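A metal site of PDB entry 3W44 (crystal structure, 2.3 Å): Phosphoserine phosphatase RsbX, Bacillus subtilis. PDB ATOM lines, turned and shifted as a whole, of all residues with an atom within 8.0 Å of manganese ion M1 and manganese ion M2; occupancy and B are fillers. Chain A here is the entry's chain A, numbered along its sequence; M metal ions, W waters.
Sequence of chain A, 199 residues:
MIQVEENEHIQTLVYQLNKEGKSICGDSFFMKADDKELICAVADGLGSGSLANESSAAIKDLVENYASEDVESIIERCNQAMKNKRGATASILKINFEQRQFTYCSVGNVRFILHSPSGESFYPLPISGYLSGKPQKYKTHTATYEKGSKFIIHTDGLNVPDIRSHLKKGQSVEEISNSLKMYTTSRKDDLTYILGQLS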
ATOM      1  N   LYS A  19     -23.507  -8.272  28.715  1.00  0.00           N
ATOM      2  CA  LYS A  19     -22.706  -7.154  29.171  1.00  0.00           C
ATOM      3  C   LYS A  19     -23.168  -6.760  30.576  1.00  0.00           C
ATOM      4  O   LYS A  19     -24.331  -6.812  30.848  1.00  0.00           O
ATOM      5  CB  LYS A  19     -22.906  -5.990  28.205  1.00  0.00           C
ATOM      6  CG  LYS A  19     -22.248  -4.705  28.647  1.00  0.00           C
ATOM      7  CD  LYS A  19     -22.237  -3.629  27.596  1.00  0.00           C
ATOM      8  CE  LYS A  19     -21.292  -2.502  28.031  1.00  0.00           C
ATOM      9  NZ  LYS A  19     -21.370  -1.334  27.107  1.00  0.00           N
ATOM     10  N   CYS A  25     -29.171  -9.630  25.997  1.00  0.00           N
ATOM     11  CA  CYS A  25     -27.918  -9.840  25.282  1.00  0.00           C
ATOM     12  C   CYS A  25     -27.956  -9.164  23.899  1.00  0.00           C
ATOM     13  O   CYS A  25     -28.804  -9.495  23.084  1.00  0.00           O
ATOM     14  CB  CYS A  25     -27.641 -11.352  25.141  1.00  0.00           C
ATOM     15  SG  CYS A  25     -25.867 -11.623  24.870  1.00  0.00           S
ATOM     16  N   GLY A  26     -27.049  -8.221  23.661  1.00  0.00           N
ATOM     17  CA  GLY A  26     -26.771  -7.778  22.302  1.00  0.00           C
ATOM     18  C   GLY A  26     -26.347  -8.868  21.303  1.00  0.00           C
ATOM     19  O   GLY A  26     -26.604  -8.712  20.108  1.00  0.00           O
ATOM     20  N   ASP A  27     -25.708  -9.965  21.758  1.00  0.00           N
ATOM     21  CA  ASP A  27     -25.355 -11.136  20.904  1.00  0.00           C
ATOM     22  C   ASP A  27     -26.505 -12.080  20.714  1.00  0.00           C
ATOM     23  O   ASP A  27     -27.347 -12.158  21.566  1.00  0.00           O
ATOM     24  CB  ASP A  27     -24.223 -11.944  21.501  1.00  0.00           C
ATOM     25  CG  ASP A  27     -22.909 -11.143  21.618  1.00  0.00           C
ATOM     26  OD1 ASP A  27     -22.851  -9.997  21.139  1.00  0.00           O
ATOM     27  OD2 ASP A  27     -21.922 -11.667  22.210  1.00  0.00           O
ATOM     28  N   ALA A  43     -24.252 -13.980  16.173  1.00  0.00           N
ATOM     29  CA  ALA A  43     -24.333 -12.607  15.698  1.00  0.00           C
ATOM     30  C   ALA A  43     -24.140 -11.670  16.889  1.00  0.00           C
ATOM     31  O   ALA A  43     -24.527 -11.982  17.998  1.00  0.00           O
ATOM     32  CB  ALA A  43     -25.665 -12.362  15.039  1.00  0.00           C
ATOM     33  N   ASP A  44     -23.497 -10.551  16.647  1.00  0.00           N
ATOM     34  CA  ASP A  44     -23.226  -9.562  17.636  1.00  0.00           C
ATOM     35  C   ASP A  44     -23.873  -8.275  17.126  1.00  0.00           C
ATOM     36  O   ASP A  44     -23.303  -7.616  16.267  1.00  0.00           O
ATOM     37  CB  ASP A  44     -21.726  -9.408  17.670  1.00  0.00           C
ATOM     38  CG  ASP A  44     -21.261  -8.329  18.590  1.00  0.00           C
ATOM     39  OD1 ASP A  44     -22.116  -7.588  19.035  1.00  0.00           O
ATOM     40  OD2 ASP A  44     -20.054  -8.221  18.892  1.00  0.00           O
ATOM     41  N   GLY A  45     -25.017  -7.887  17.644  1.00  0.00           N
ATOM     42  CA  GLY A  45     -25.652  -6.592  17.227  1.00  0.00           C
ATOM     43  C   GLY A  45     -24.728  -5.438  17.605  1.00  0.00           C
ATOM     44  O   GLY A  45     -24.113  -5.505  18.656  1.00  0.00           O
ATOM     45  N   LEU A  46     -24.609  -4.420  16.748  1.00  0.00           N
ATOM     46  CA  LEU A  46     -23.801  -3.236  17.013  1.00  0.00           C
ATOM     47  C   LEU A  46     -24.158  -2.628  18.353  1.00  0.00           C
ATOM     48  O   LEU A  46     -25.334  -2.442  18.604  1.00  0.00           O
ATOM     49  CB  LEU A  46     -23.927  -2.187  15.882  1.00  0.00           C
ATOM     50  CG  LEU A  46     -22.676  -2.292  14.990  1.00  0.00           C
ATOM     51  CD1 LEU A  46     -22.631  -3.660  14.304  1.00  0.00           C
ATOM     52  CD2 LEU A  46     -22.452  -1.146  13.939  1.00  0.00           C
ATOM     53  N   GLY A  47     -23.171  -2.353  19.204  1.00  0.00           N
ATOM     54  CA  GLY A  47     -23.411  -1.771  20.503  1.00  0.00           C
ATOM     55  C   GLY A  47     -23.914  -2.869  21.406  1.00  0.00           C
ATOM     56  O   GLY A  47     -23.529  -4.053  21.275  1.00  0.00           O
ATOM     57  N   SER A  48     -24.767  -2.510  22.352  1.00  0.00           N
ATOM     58  CA  SER A  48     -25.488  -3.558  23.101  1.00  0.00           C
ATOM     59  C   SER A  48     -26.897  -3.038  23.463  1.00  0.00           C
ATOM     60  O   SER A  48     -27.386  -2.036  22.897  1.00  0.00           O
ATOM     61  CB  SER A  48     -24.669  -4.042  24.298  1.00  0.00           C
ATOM     62  OG  SER A  48     -24.120  -2.898  24.935  1.00  0.00           O
ATOM     63  N   GLY A  49     -27.555  -3.710  24.396  1.00  0.00           N
ATOM     64  CA  GLY A  49     -28.856  -3.299  24.733  1.00  0.00           C
ATOM     65  C   GLY A  49     -29.801  -3.925  23.760  1.00  0.00           C
ATOM     66  O   GLY A  49     -29.450  -4.845  22.956  1.00  0.00           O
ATOM     67  N   ALA A  52     -29.299  -3.512  19.965  1.00  0.00           N
ATOM     68  CA  ALA A  52     -28.316  -4.494  19.500  1.00  0.00           C
ATOM     69  C   ALA A  52     -28.974  -5.891  19.390  1.00  0.00           C
ATOM     70  O   ALA A  52     -28.792  -6.619  18.419  1.00  0.00           O
ATOM     71  CB  ALA A  52     -27.089  -4.536  20.423  1.00  0.00           C
ATOM     72  N   ASN A  53     -29.795  -6.228  20.358  1.00  0.00           N
ATOM     73  CA  ASN A  53     -30.452  -7.493  20.345  1.00  0.00           C
ATOM     74  C   ASN A  53     -31.505  -7.538  19.289  1.00  0.00           C
ATOM     75  O   ASN A  53     -31.716  -8.593  18.691  1.00  0.00           O
ATOM     76  CB  ASN A  53     -31.039  -7.802  21.711  1.00  0.00           C
ATOM     77  CG  ASN A  53     -31.934  -9.028  21.674  1.00  0.00           C
ATOM     78  OD1 ASN A  53     -33.072  -8.938  21.238  1.00  0.00           O
ATOM     79  ND2 ASN A  53     -31.416 -10.175  22.130  1.00  0.00           N
ATOM     80  N   SER A  56     -29.451  -8.631  16.341  1.00  0.00           N
ATOM     81  CA  SER A  56     -28.972  -9.988  16.445  1.00  0.00           C
ATOM     82  C   SER A  56     -30.038 -11.090  16.550  1.00  0.00           C
ATOM     83  O   SER A  56     -29.869 -12.153  15.955  1.00  0.00           O
ATOM     84  CB  SER A  56     -27.876 -10.122  17.507  1.00  0.00           C
ATOM     85  OG  SER A  56     -28.456 -10.025  18.763  1.00  0.00           O
ATOM     86  N   ARG A  86     -29.716  -1.386  13.762  1.00  0.00           N
ATOM     87  CA  ARG A  86     -28.337  -1.104  14.079  1.00  0.00           C
ATOM     88  C   ARG A  86     -27.340  -1.862  13.207  1.00  0.00           C
ATOM     89  O   ARG A  86     -26.272  -1.326  12.925  1.00  0.00           O
ATOM     90  CB  ARG A  86     -28.032  -1.469  15.499  1.00  0.00           C
ATOM     91  CG  ARG A  86     -28.270  -0.294  16.377  1.00  0.00           C
ATOM     92  CD  ARG A  86     -27.370  -0.293  17.515  1.00  0.00           C
ATOM     93  NE  ARG A  86     -27.966   0.587  18.498  1.00  0.00           N
ATOM     94  CZ  ARG A  86     -27.939   0.368  19.811  1.00  0.00           C
ATOM     95  NH1 ARG A  86     -27.322  -0.706  20.309  1.00  0.00           N
ATOM     96  NH2 ARG A  86     -28.509   1.262  20.616  1.00  0.00           N
ATOM     97  N   GLY A  87     -27.670  -3.101  12.800  1.00  0.00           N
ATOM     98  CA  GLY A  87     -26.716  -3.932  12.060  1.00  0.00           C
ATOM     99  C   GLY A  87     -26.038  -4.862  13.022  1.00  0.00           C
ATOM    100  O   GLY A  87     -26.250  -4.782  14.240  1.00  0.00           O
ATOM    101  N   ALA A  88     -25.230  -5.769  12.503  1.00  0.00           N
ATOM    102  CA  ALA A  88     -24.621  -6.784  13.356  1.00  0.00           C
ATOM    103  C   ALA A  88     -23.436  -7.417  12.626  1.00  0.00           C
ATOM    104  O   ALA A  88     -23.410  -7.417  11.447  1.00  0.00           O
ATOM    105  CB  ALA A  88     -25.668  -7.819  13.660  1.00  0.00           C
ATOM    106  N   THR A  89     -22.486  -7.999  13.357  1.00  0.00           N
ATOM    107  CA  THR A  89     -21.520  -8.884  12.754  1.00  0.00           C
ATOM    108  C   THR A  89     -22.028 -10.305  12.951  1.00  0.00           C
ATOM    109  O   THR A  89     -22.732 -10.567  13.863  1.00  0.00           O
ATOM    110  CB  THR A  89     -20.151  -8.639  13.330  1.00  0.00           C
ATOM    111  OG1 THR A  89     -20.212  -8.768  14.737  1.00  0.00           O
ATOM    112  CG2 THR A  89     -19.732  -7.170  13.020  1.00  0.00           C
ATOM    113  N   ASN A 109     -16.334  -8.885  12.747  1.00  0.00           N
ATOM    114  CA  ASN A 109     -15.465  -9.534  13.682  1.00  0.00           C
ATOM    115  C   ASN A 109     -16.089 -10.623  14.541  1.00  0.00           C
ATOM    116  O   ASN A 109     -15.999 -10.552  15.765  1.00  0.00           O
ATOM    117  CB  ASN A 109     -14.756  -8.492  14.579  1.00  0.00           C
ATOM    118  CG  ASN A 109     -13.555  -9.081  15.326  1.00  0.00           C
ATOM    119  OD1 ASN A 109     -13.147 -10.189  15.051  1.00  0.00           O
ATOM    120  ND2 ASN A 109     -13.013  -8.359  16.273  1.00  0.00           N
ATOM    121  N   VAL A 110     -16.762 -11.595  13.968  1.00  0.00           N
ATOM    122  CA  VAL A 110     -17.101 -12.803  14.710  1.00  0.00           C
ATOM    123  C   VAL A 110     -16.110 -13.855  14.209  1.00  0.00           C
ATOM    124  O   VAL A 110     -15.893 -13.943  12.988  1.00  0.00           O
ATOM    125  CB  VAL A 110     -18.575 -13.209  14.504  1.00  0.00           C
ATOM    126  CG1 VAL A 110     -18.909 -14.527  15.312  1.00  0.00           C
ATOM    127  CG2 VAL A 110     -19.450 -12.098  15.005  1.00  0.00           C
ATOM    128  N   THR A 155     -18.082 -14.161  19.526  1.00  0.00           N
ATOM    129  CA  THR A 155     -18.091 -12.746  19.380  1.00  0.00           C
ATOM    130  C   THR A 155     -16.851 -12.077  20.007  1.00  0.00           C
ATOM    131  O   THR A 155     -16.020 -12.730  20.684  1.00  0.00           O
ATOM    132  CB  THR A 155     -19.360 -12.142  19.974  1.00  0.00           C
ATOM    133  OG1 THR A 155     -19.404 -12.488  21.333  1.00  0.00           O
ATOM    134  CG2 THR A 155     -20.604 -12.681  19.346  1.00  0.00           C
ATOM    135  N   ASP A 156     -16.678 -10.776  19.758  1.00  0.00           N
ATOM    136  CA  ASP A 156     -15.452 -10.081  20.116  1.00  0.00           C
ATOM    137  C   ASP A 156     -15.404  -9.817  21.608  1.00  0.00           C
ATOM    138  O   ASP A 156     -14.406  -9.362  22.119  1.00  0.00           O
ATOM    139  CB  ASP A 156     -15.311  -8.761  19.353  1.00  0.00           C
ATOM    140  CG  ASP A 156     -16.522  -7.824  19.549  1.00  0.00           C
ATOM    141  OD1 ASP A 156     -17.352  -8.029  20.453  1.00  0.00           O
ATOM    142  OD2 ASP A 156     -16.631  -6.853  18.754  1.00  0.00           O
ATOM    143  N   GLY A 157     -16.472 -10.107  22.325  1.00  0.00           N
ATOM    144  CA  GLY A 157     -16.403 -10.088  23.790  1.00  0.00           C
ATOM    145  C   GLY A 157     -15.464 -11.093  24.457  1.00  0.00           C
ATOM    146  O   GLY A 157     -15.112 -10.948  25.647  1.00  0.00           O
ATOM    147  N   LEU A 158     -15.103 -12.123  23.729  1.00  0.00           N
ATOM    148  CA  LEU A 158     -14.232 -13.150  24.274  1.00  0.00           C
ATOM    149  C   LEU A 158     -12.875 -12.782  23.753  1.00  0.00           C
ATOM    150  O   LEU A 158     -12.653 -12.815  22.517  1.00  0.00           O
ATOM    151  CB  LEU A 158     -14.607 -14.538  23.737  1.00  0.00           C
ATOM    152  CG  LEU A 158     -13.724 -15.708  24.170  1.00  0.00           C
ATOM    153  CD1 LEU A 158     -13.922 -15.989  25.697  1.00  0.00           C
ATOM    154  CD2 LEU A 158     -14.010 -16.975  23.336  1.00  0.00           C
ATOM    155  N   LYS A 188     -17.258  -6.687  30.191  1.00  0.00           N
ATOM    156  CA  LYS A 188     -17.062  -5.452  29.470  1.00  0.00           C
ATOM    157  C   LYS A 188     -17.988  -5.435  28.244  1.00  0.00           C
ATOM    158  O   LYS A 188     -18.419  -4.367  27.793  1.00  0.00           O
ATOM    159  CB  LYS A 188     -15.593  -5.247  29.099  1.00  0.00           C
ATOM    160  CG  LYS A 188     -14.686  -5.063  30.340  1.00  0.00           C
ATOM    161  CD  LYS A 188     -13.627  -3.982  30.161  1.00  0.00           C
ATOM    162  CE  LYS A 188     -13.293  -3.340  31.525  1.00  0.00           C
ATOM    163  NZ  LYS A 188     -14.532  -2.869  32.283  1.00  0.00           N
ATOM    164  N   ASP A 189     -18.367  -6.617  27.738  1.00  0.00           N
ATOM    165  CA  ASP A 189     -19.194  -6.680  26.545  1.00  0.00           C
ATOM    166  C   ASP A 189     -20.028  -7.930  26.657  1.00  0.00           C
ATOM    167  O   ASP A 189     -19.744  -8.740  27.479  1.00  0.00           O
ATOM    168  CB  ASP A 189     -18.265  -6.731  25.338  1.00  0.00           C
ATOM    169  CG  ASP A 189     -18.978  -6.662  24.001  1.00  0.00           C
ATOM    170  OD1 ASP A 189     -20.181  -6.349  23.888  1.00  0.00           O
ATOM    171  OD2 ASP A 189     -18.291  -6.936  23.031  1.00  0.00           O
ATOM    172  N   ASP A 190     -21.051  -8.065  25.831  1.00  0.00           N
ATOM    173  CA  ASP A 190     -21.741  -9.302  25.678  1.00  0.00           C
ATOM    174  C   ASP A 190     -20.712 -10.323  25.193  1.00  0.00           C
ATOM    175  O   ASP A 190     -19.829  -9.968  24.438  1.00  0.00           O
ATOM    176  CB  ASP A 190     -22.864  -9.184  24.618  1.00  0.00           C
ATOM    177  CG  ASP A 190     -23.941  -8.174  24.983  1.00  0.00           C
ATOM    178  OD1 ASP A 190     -24.533  -8.266  26.060  1.00  0.00           O
ATOM    179  OD2 ASP A 190     -24.261  -7.300  24.154  1.00  0.00           O
ATOM    180  N   LEU A 191     -20.884 -11.586  25.529  1.00  0.00           N
ATOM    181  CA  LEU A 191     -19.904 -12.602  25.231  1.00  0.00           C
ATOM    182  C   LEU A 191     -20.608 -13.873  24.854  1.00  0.00           C
ATOM    183  O   LEU A 191     -21.321 -14.407  25.633  1.00  0.00           O
ATOM    184  CB  LEU A 191     -18.955 -12.804  26.439  1.00  0.00           C
ATOM    185  CG  LEU A 191     -17.624 -13.550  26.205  1.00  0.00           C
ATOM    186  CD1 LEU A 191     -16.807 -13.446  27.358  1.00  0.00           C
ATOM    187  CD2 LEU A 191     -17.779 -14.994  25.987  1.00  0.00           C
ATOM    188  N   THR A 192     -20.423 -14.339  23.622  1.00  0.00           N
ATOM    189  CA  THR A 192     -21.095 -15.548  23.130  1.00  0.00           C
ATOM    190  C   THR A 192     -20.059 -16.408  22.462  1.00  0.00           C
ATOM    191  O   THR A 192     -19.281 -15.902  21.665  1.00  0.00           O
ATOM    192  CB  THR A 192     -22.120 -15.185  22.097  1.00  0.00           C
ATOM    193  OG1 THR A 192     -23.083 -14.386  22.711  1.00  0.00           O
ATOM    194  CG2 THR A 192     -22.835 -16.385  21.470  1.00  0.00           C
HETATM  195 MN    MN M   1     -22.646  -5.814  20.200  1.00  0.00          MN
HETATM  196 MN    MN M   2     -19.297  -7.318  20.936  1.00  0.00          MN
HETATM  197  O   HOH W   1     -21.154  -4.662  18.885  1.00  0.00           O
HETATM  198  O   HOH W   2     -23.678  -7.450  21.368  1.00  0.00           O
HETATM  199  O   HOH W   3     -18.739  -5.454  19.629  1.00  0.00           O
HETATM  200  O   HOH W   4     -21.000  -5.864  21.403  1.00  0.00           O
HETATM  201  O   HOH W   5     -20.546  -9.050  21.777  1.00  0.00           O
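Manganese ion M2 is bound by OD1 of Asp 156 (2.1 Å), water W4 (2.3 Å), water W5 (2.3 Å), water W3 (2.3 Å), OD2 of Asp 189 (2.4 Å) and OD2 of Asp 44 (2.4 Å).
C of Leu 46 touches manganese ion M1, 3.98 Å away.
Of the 29 residues printed, 4 come within 4 Å of manganese ion M1.
The nearest printed residue that does not touch manganese ion M1 is Asp 27 (4.3 Å).
The backbone NH of Gly 45 sits at hydrogen-bond distance from the backbone carbonyl oxygen of Gly 26 (3.0 Å).
The backbone NH (N) of Leu 46 lies within hydrogen-bond range of the backbone carbonyl oxygen (O) of Gly 87 (3.0 Å).
O of Leu 46 is in hydrogen-bond range of NH1 of Arg 86 (3.1 Å).
N of Asp 44 sits at hydrogen-bond distance from O of Thr 89 (2.9 Å).
Manganese ion M1 is bound by water W4 (2.0 Å), O of Gly 45 (2.2 Å), OD1 of Asp 44 (2.2 Å), O of Gly 47 (2.2 Å), water W2 (2.3 Å) and water W1 (2.3 Å).
Three residues have an atom within 4 Å of manganese ion M2: Asp 44, Asp 156 and Asp 189.
Along chain A the residues within 4 Å of manganese ion M2 span positions 44 to 189.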
